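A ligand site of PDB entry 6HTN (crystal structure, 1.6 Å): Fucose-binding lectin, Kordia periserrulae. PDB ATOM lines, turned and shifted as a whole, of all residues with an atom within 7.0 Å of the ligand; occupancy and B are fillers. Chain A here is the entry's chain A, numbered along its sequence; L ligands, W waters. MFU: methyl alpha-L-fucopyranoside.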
ATOM      1  N   TRP A   6      27.031  28.540   8.201  1.00  0.00           N
ATOM      2  CA  TRP A   6      27.138  29.847   8.898  1.00  0.00           C
ATOM      3  C   TRP A   6      28.151  29.708  10.017  1.00  0.00           C
ATOM      4  O   TRP A   6      28.400  28.606  10.500  1.00  0.00           O
ATOM      5  CB  TRP A   6      25.802  30.351   9.422  1.00  0.00           C
ATOM      6  CG  TRP A   6      25.206  29.507  10.506  1.00  0.00           C
ATOM      7  CD1 TRP A   6      25.314  29.708  11.862  1.00  0.00           C
ATOM      8  CD2 TRP A   6      24.461  28.296  10.360  1.00  0.00           C
ATOM      9  NE1 TRP A   6      24.658  28.730  12.559  1.00  0.00           N
ATOM     10  CE2 TRP A   6      24.087  27.861  11.661  1.00  0.00           C
ATOM     11  CE3 TRP A   6      23.971  27.580   9.238  1.00  0.00           C
ATOM     12  CZ2 TRP A   6      23.330  26.722  11.880  1.00  0.00           C
ATOM     13  CZ3 TRP A   6      23.161  26.504   9.470  1.00  0.00           C
ATOM     14  CH2 TRP A   6      22.876  26.045  10.763  1.00  0.00           C
ATOM     15  N   LEU A  15      27.319  23.368   9.281  1.00  0.00           N
ATOM     16  CA  LEU A  15      26.992  22.948   7.882  1.00  0.00           C
ATOM     17  C   LEU A  15      25.643  22.294   7.902  1.00  0.00           C
ATOM     18  O   LEU A  15      25.328  21.501   8.824  1.00  0.00           O
ATOM     19  CB  LEU A  15      28.055  21.968   7.366  1.00  0.00           C
ATOM     20  CG  LEU A  15      29.511  22.394   7.417  1.00  0.00           C
ATOM     21  CD1 LEU A  15      30.432  21.239   6.972  1.00  0.00           C
ATOM     22  CD2 LEU A  15      29.769  23.598   6.523  1.00  0.00           C
ATOM     23  N   ARG A  16      24.845  22.550   6.873  1.00  0.00           N
ATOM     24  CA  ARG A  16      23.561  21.857   6.677  1.00  0.00           C
ATOM     25  C   ARG A  16      23.526  21.375   5.218  1.00  0.00           C
ATOM     26  O   ARG A  16      23.587  22.251   4.319  1.00  0.00           O
ATOM     27  CB  ARG A  16      22.343  22.668   7.038  1.00  0.00           C
ATOM     28  CG  ARG A  16      22.315  23.119   8.502  1.00  0.00           C
ATOM     29  CD  ARG A  16      22.020  21.919   9.415  1.00  0.00           C
ATOM     30  NE  ARG A  16      21.909  22.367  10.835  1.00  0.00           N
ATOM     31  CZ  ARG A  16      22.908  22.480  11.688  1.00  0.00           C
ATOM     32  NH1 ARG A  16      24.147  22.294  11.349  1.00  0.00           N
ATOM     33  NH2 ARG A  16      22.635  22.840  12.926  1.00  0.00           N
ATOM     34  N   TYR A  18      21.509  19.083   2.319  1.00  0.00           N
ATOM     35  CA  TYR A  18      20.174  18.590   1.986  1.00  0.00           C
ATOM     36  C   TYR A  18      20.239  17.709   0.736  1.00  0.00           C
ATOM     37  O   TYR A  18      20.851  18.118  -0.280  1.00  0.00           O
ATOM     38  CB  TYR A  18      19.208  19.765   1.764  1.00  0.00           C
ATOM     39  CG  TYR A  18      19.081  20.639   3.001  1.00  0.00           C
ATOM     40  CD1 TYR A  18      18.210  20.300   4.038  1.00  0.00           C
ATOM     41  CD2 TYR A  18      19.915  21.724   3.169  1.00  0.00           C
ATOM     42  CE1 TYR A  18      18.171  21.051   5.201  1.00  0.00           C
ATOM     43  CE2 TYR A  18      19.873  22.487   4.312  1.00  0.00           C
ATOM     44  CZ  TYR A  18      18.998  22.150   5.336  1.00  0.00           C
ATOM     45  OH  TYR A  18      19.047  22.859   6.532  1.00  0.00           O
ATOM     46  N   GLU A  29      18.368  15.873   5.878  1.00  0.00           N
ATOM     47  CA  GLU A  29      19.206  16.995   6.332  1.00  0.00           C
ATOM     48  C   GLU A  29      20.353  16.438   7.151  1.00  0.00           C
ATOM     49  O   GLU A  29      20.049  15.714   8.167  1.00  0.00           O
ATOM     50  CB  GLU A  29      18.403  17.975   7.171  1.00  0.00           C
ATOM     51  CG  GLU A  29      19.237  19.110   7.726  1.00  0.00           C
ATOM     52  CD  GLU A  29      18.480  20.000   8.682  1.00  0.00           C
ATOM     53  OE1 GLU A  29      17.671  19.472   9.504  1.00  0.00           O
ATOM     54  OE2 GLU A  29      18.654  21.268   8.608  1.00  0.00           O
ATOM     55  N   CYS A  31      23.783  17.369   9.366  1.00  0.00           N
ATOM     56  CA  CYS A  31      24.232  18.544  10.146  1.00  0.00           C
ATOM     57  C   CYS A  31      25.610  18.361  10.714  1.00  0.00           C
ATOM     58  O   CYS A  31      25.921  17.257  11.216  1.00  0.00           O
ATOM     59  CB  CYS A  31      23.292  18.775  11.309  1.00  0.00           C
ATOM     60  SG  CYS A  31      21.556  18.895  10.914  1.00  0.00           S
ATOM     61  N   ASP A  33      27.954  20.543  13.540  1.00  0.00           N
ATOM     62  CA  ASP A  33      28.008  21.702  14.469  1.00  0.00           C
ATOM     63  C   ASP A  33      29.348  21.790  15.181  1.00  0.00           C
ATOM     64  O   ASP A  33      29.659  22.908  15.688  1.00  0.00           O
ATOM     65  CB  ASP A  33      26.921  21.636  15.522  1.00  0.00           C
ATOM     66  CG  ASP A  33      25.522  21.784  14.990  1.00  0.00           C
ATOM     67  OD1 ASP A  33      25.341  22.634  14.088  1.00  0.00           O
ATOM     68  OD2 ASP A  33      24.650  21.213  15.580  1.00  0.00           O
ATOM     69  N   TYR A  38      25.268  14.493  11.924  1.00  0.00           N
ATOM     70  CA  TYR A  38      24.047  13.887  12.473  1.00  0.00           C
ATOM     71  C   TYR A  38      22.837  14.234  11.635  1.00  0.00           C
ATOM     72  O   TYR A  38      22.893  15.181  10.783  1.00  0.00           O
ATOM     73  CB  TYR A  38      23.933  14.308  13.940  1.00  0.00           C
ATOM     74  CG  TYR A  38      23.569  15.751  14.194  1.00  0.00           C
ATOM     75  CD1 TYR A  38      22.268  16.181  14.234  1.00  0.00           C
ATOM     76  CD2 TYR A  38      24.582  16.671  14.388  1.00  0.00           C
ATOM     77  CE1 TYR A  38      21.944  17.515  14.446  1.00  0.00           C
ATOM     78  CE2 TYR A  38      24.279  18.023  14.643  1.00  0.00           C
ATOM     79  CZ  TYR A  38      22.955  18.441  14.665  1.00  0.00           C
ATOM     80  OH  TYR A  38      22.600  19.744  14.849  1.00  0.00           O
ATOM     81  N   ASP A  39      21.766  13.537  11.820  1.00  0.00           N
ATOM     82  CA  ASP A  39      20.518  13.788  11.086  1.00  0.00           C
ATOM     83  C   ASP A  39      19.802  14.980  11.697  1.00  0.00           C
ATOM     84  O   ASP A  39      19.435  14.984  12.902  1.00  0.00           O
ATOM     85  CB  ASP A  39      19.558  12.604  11.061  1.00  0.00           C
ATOM     86  CG  ASP A  39      19.996  11.415  10.231  1.00  0.00           C
ATOM     87  OD1 ASP A  39      20.997  11.504   9.471  1.00  0.00           O
ATOM     88  OD2 ASP A  39      19.398  10.308  10.523  1.00  0.00           O
ATOM     89  N   GLY A  40      19.469  15.981  10.887  1.00  0.00           N
ATOM     90  CA  GLY A  40      18.682  17.112  11.325  1.00  0.00           C
ATOM     91  C   GLY A  40      17.203  16.849  11.375  1.00  0.00           C
ATOM     92  O   GLY A  40      16.711  15.851  10.780  1.00  0.00           O
ATOM     93  N   ALA A  41      16.443  17.732  11.986  1.00  0.00           N
ATOM     94  CA  ALA A  41      15.011  17.614  12.219  1.00  0.00           C
ATOM     95  C   ALA A  41      14.210  17.515  10.913  1.00  0.00           C
ATOM     96  O   ALA A  41      13.116  16.998  10.902  1.00  0.00           O
ATOM     97  CB  ALA A  41      14.533  18.737  13.092  1.00  0.00           C
ATOM     98  N   LEU A  42      14.732  18.116   9.814  1.00  0.00           N
ATOM     99  CA  LEU A  42      13.963  18.077   8.541  1.00  0.00           C
ATOM    100  C   LEU A  42      13.834  16.620   8.044  1.00  0.00           C
ATOM    101  O   LEU A  42      12.873  16.331   7.360  1.00  0.00           O
ATOM    102  CB  LEU A  42      14.666  18.983   7.515  1.00  0.00           C
ATOM    103  CG  LEU A  42      14.112  18.920   6.092  1.00  0.00           C
ATOM    104  CD1 LEU A  42      14.255  20.308   5.421  1.00  0.00           C
ATOM    105  CD2 LEU A  42      14.853  17.854   5.282  1.00  0.00           C
ATOM    106  N   THR A  43      14.804  15.792   8.399  1.00  0.00           N
ATOM    107  CA  THR A  43      14.958  14.429   7.832  1.00  0.00           C
ATOM    108  C   THR A  43      13.652  13.639   7.908  1.00  0.00           C
ATOM    109  O   THR A  43      13.046  13.546   8.996  1.00  0.00           O
ATOM    110  CB  THR A  43      16.063  13.687   8.548  1.00  0.00           C
ATOM    111  OG1 THR A  43      17.269  14.383   8.338  1.00  0.00           O
ATOM    112  CG2 THR A  43      16.224  12.248   8.099  1.00  0.00           C
ATOM    113  N   GLN A  45      10.693  14.111   6.883  1.00  0.00           N
ATOM    114  CA  GLN A  45       9.394  14.765   7.008  1.00  0.00           C
ATOM    115  C   GLN A  45       8.726  15.015   5.662  1.00  0.00           C
ATOM    116  O   GLN A  45       7.480  15.064   5.613  1.00  0.00           O
ATOM    117  CB  GLN A  45       9.456  16.093   7.745  1.00  0.00           C
ATOM    118  CG  GLN A  45       9.820  16.000   9.213  1.00  0.00           C
ATOM    119  CD  GLN A  45       9.482  17.329   9.886  1.00  0.00           C
ATOM    120  OE1 GLN A  45       8.357  17.821   9.806  1.00  0.00           O
ATOM    121  NE2 GLN A  45      10.498  17.980  10.458  1.00  0.00           N
ATOM    122  N   GLN A  63      20.200  34.098  15.653  1.00  0.00           N
ATOM    123  CA  GLN A  63      19.317  32.958  15.307  1.00  0.00           C
ATOM    124  C   GLN A  63      19.463  32.665  13.812  1.00  0.00           C
ATOM    125  O   GLN A  63      19.266  33.592  13.014  1.00  0.00           O
ATOM    126  CB  GLN A  63      17.865  33.236  15.652  1.00  0.00           C
ATOM    127  CG  GLN A  63      16.904  32.147  15.166  1.00  0.00           C
ATOM    128  CD  GLN A  63      17.141  30.786  15.785  1.00  0.00           C
ATOM    129  OE1 GLN A  63      17.167  30.629  17.022  1.00  0.00           O
ATOM    130  NE2 GLN A  63      17.355  29.761  14.957  1.00  0.00           N
ATOM    131  N   ILE A  64      19.786  31.426  13.478  1.00  0.00           N
ATOM    132  CA  ILE A  64      19.853  30.988  12.050  1.00  0.00           C
ATOM    133  C   ILE A  64      18.464  30.831  11.511  1.00  0.00           C
ATOM    134  O   ILE A  64      17.535  30.280  12.175  1.00  0.00           O
ATOM    135  CB  ILE A  64      20.729  29.750  11.894  1.00  0.00           C
ATOM    136  CG1 ILE A  64      21.052  29.456  10.431  1.00  0.00           C
ATOM    137  CG2 ILE A  64      20.051  28.537  12.525  1.00  0.00           C
ATOM    138  CD1 ILE A  64      21.940  30.494   9.800  1.00  0.00           C
ATOM    139  N   HIS A  65      18.263  31.236  10.243  1.00  0.00           N
ATOM    140  CA  HIS A  65      17.046  31.003   9.479  1.00  0.00           C
ATOM    141  C   HIS A  65      17.478  30.232   8.221  1.00  0.00           C
ATOM    142  O   HIS A  65      18.529  30.616   7.645  1.00  0.00           O
ATOM    143  CB  HIS A  65      16.367  32.301   9.043  1.00  0.00           C
ATOM    144  CG  HIS A  65      15.985  33.138  10.225  1.00  0.00           C
ATOM    145  ND1 HIS A  65      14.659  33.214  10.611  1.00  0.00           N
ATOM    146  CD2 HIS A  65      16.721  33.900  11.060  1.00  0.00           C
ATOM    147  CE1 HIS A  65      14.606  34.014  11.721  1.00  0.00           C
ATOM    148  NE2 HIS A  65      15.850  34.401  12.020  1.00  0.00           N
ATOM    149  N   ILE A  66      16.737  29.193   7.870  1.00  0.00           N
ATOM    150  CA  ILE A  66      17.119  28.370   6.706  1.00  0.00           C
ATOM    151  C   ILE A  66      15.912  28.255   5.799  1.00  0.00           C
ATOM    152  O   ILE A  66      14.775  28.128   6.245  1.00  0.00           O
ATOM    153  CB  ILE A  66      17.612  26.973   7.145  1.00  0.00           C
ATOM    154  CG1 ILE A  66      18.714  27.037   8.176  1.00  0.00           C
ATOM    155  CG2 ILE A  66      18.019  26.155   5.922  1.00  0.00           C
ATOM    156  CD1 ILE A  66      19.099  25.690   8.793  1.00  0.00           C
ATOM    157  N   TRP A  82      12.885  27.103   8.312  1.00  0.00           N
ATOM    158  CA  TRP A  82      13.300  27.012   9.735  1.00  0.00           C
ATOM    159  C   TRP A  82      13.595  28.427  10.205  1.00  0.00           C
ATOM    160  O   TRP A  82      14.470  29.094   9.627  1.00  0.00           O
ATOM    161  CB  TRP A  82      14.510  26.127   9.880  1.00  0.00           C
ATOM    162  CG  TRP A  82      15.032  26.006  11.288  1.00  0.00           C
ATOM    163  CD1 TRP A  82      15.879  26.831  11.946  1.00  0.00           C
ATOM    164  CD2 TRP A  82      14.714  24.930  12.181  1.00  0.00           C
ATOM    165  NE1 TRP A  82      16.110  26.347  13.212  1.00  0.00           N
ATOM    166  CE2 TRP A  82      15.399  25.196  13.384  1.00  0.00           C
ATOM    167  CE3 TRP A  82      13.880  23.820  12.098  1.00  0.00           C
ATOM    168  CZ2 TRP A  82      15.330  24.304  14.462  1.00  0.00           C
ATOM    169  CZ3 TRP A  82      13.817  22.950  13.172  1.00  0.00           C
ATOM    170  CH2 TRP A  82      14.530  23.209  14.335  1.00  0.00           C
ATOM    171  N   LYS A  84      13.428  28.918  14.032  1.00  0.00           N
ATOM    172  CA  LYS A  84      13.735  28.819  15.470  1.00  0.00           C
ATOM    173  C   LYS A  84      13.720  27.364  15.909  1.00  0.00           C
ATOM    174  O   LYS A  84      14.735  26.954  16.445  1.00  0.00           O
ATOM    175  CB  LYS A  84      12.727  29.642  16.283  1.00  0.00           C
ATOM    176  CG  LYS A  84      12.952  29.618  17.798  1.00  0.00           C
ATOM    177  CD  LYS A  84      13.637  30.786  18.403  1.00  0.00           C
ATOM    178  CE  LYS A  84      14.050  30.506  19.839  1.00  0.00           C
ATOM    179  NZ  LYS A  84      12.932  30.649  20.803  1.00  0.00           N
ATOM    180  N   TRP A  87      10.325  23.003  11.288  1.00  0.00           N
ATOM    181  CA  TRP A  87      10.210  23.193   9.837  1.00  0.00           C
ATOM    182  C   TRP A  87       8.762  23.396   9.458  1.00  0.00           C
ATOM    183  O   TRP A  87       7.876  22.647   9.925  1.00  0.00           O
ATOM    184  CB  TRP A  87      10.791  21.986   9.111  1.00  0.00           C
ATOM    185  CG  TRP A  87      12.272  21.936   9.227  1.00  0.00           C
ATOM    186  CD1 TRP A  87      13.014  21.255  10.114  1.00  0.00           C
ATOM    187  CD2 TRP A  87      13.226  22.647   8.395  1.00  0.00           C
ATOM    188  NE1 TRP A  87      14.344  21.479   9.934  1.00  0.00           N
ATOM    189  CE2 TRP A  87      14.497  22.334   8.846  1.00  0.00           C
ATOM    190  CE3 TRP A  87      13.084  23.504   7.288  1.00  0.00           C
ATOM    191  CZ2 TRP A  87      15.653  22.830   8.277  1.00  0.00           C
ATOM    192  CZ3 TRP A  87      14.231  23.982   6.710  1.00  0.00           C
ATOM    193  CH2 TRP A  87      15.489  23.659   7.163  1.00  0.00           C
HETATM  194  C1  MFU L   1      19.395  21.508  14.170  1.00  0.00           C
HETATM  195  C2  MFU L   1      18.591  20.791  13.071  1.00  0.00           C
HETATM  196  C3  MFU L   1      17.454  21.573  12.508  1.00  0.00           C
HETATM  197  C4  MFU L   1      18.002  22.859  11.915  1.00  0.00           C
HETATM  198  C5  MFU L   1      18.738  23.500  13.107  1.00  0.00           C
HETATM  199  C6  MFU L   1      19.443  24.800  12.630  1.00  0.00           C
HETATM  200  O1  MFU L   1      18.402  21.731  15.099  1.00  0.00           O
HETATM  201  O2  MFU L   1      17.951  19.612  13.683  1.00  0.00           O
HETATM  202  O3  MFU L   1      16.724  20.891  11.463  1.00  0.00           O
HETATM  203  O4  MFU L   1      19.024  22.595  10.916  1.00  0.00           O
HETATM  204  O5  MFU L   1      19.876  22.732  13.538  1.00  0.00           O
HETATM  205  CM  MFU L   1      18.977  22.372  16.278  1.00  0.00           C
HETATM  206  O   HOH W   1      16.218  19.948  16.136  1.00  0.00           O
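O of Tyr 38 sits at hydrogen-bond distance from N of Cys 31.
The side-chain carboxylate of Asp 33 sits at hydrogen-bond distance from the side-chain hydroxyl of Tyr 38 (2.6 Å).
The side-chain hydroxyl (OH) of Tyr 18 lies within hydrogen-bond range of the side-chain carboxylate (OE2) of Glu 29.
O of Ala 41 sits at hydrogen-bond distance from NE2 of Gln 45 (2.8 Å).
The backbone NH (N) of Gly 40 sits close to the side-chain sulfur (SG) of Cys 31 (3.6 Å).
OD1 of Asp 33 is in salt-bridge range of NH2 of Arg 16 (3.0 Å).
The backbone NH (N) of Ala 41 is in hydrogen-bond range of the side-chain carboxylate (OE1) of Glu 29 (3.3 Å).
The side-chain hydroxyl (OG1) of Thr 43 is in hydrogen-bond range of the backbone carbonyl oxygen (O) of Gly 40, 2.9 Å away.
O3 of the ligand sits at hydrogen-bond distance from OE1 of Glu 29 (2.6 Å).
The backbone NH (N) of Ala 41 is in hydrogen-bond range of an oxygen (O2) of the ligand, 2.9 Å away.
The indole nitrogen of Trp 87 lies within hydrogen-bond range of an oxygen (O3) of the ligand (2.9 Å).
The guanidinium group (NH2) of Arg 16 is in hydrogen-bond range of an oxygen (O5) of the ligand, at 2.8 Å.
OH of Tyr 38 touches C1 of the ligand, 3.7 Å away.
Gly 40 touches the ligand.
Leu 42 touches the ligand.
Ile 64 touches the ligand (CG2 to C6, 3.8 Å).
Ile 66 touches the ligand.
Trp 82 touches the ligand.
Hydrophobic or aromatic side chains within 4 Å of the ligand: Ala 41, Ile 64, Ile 66, Trp 82 and Trp 87.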
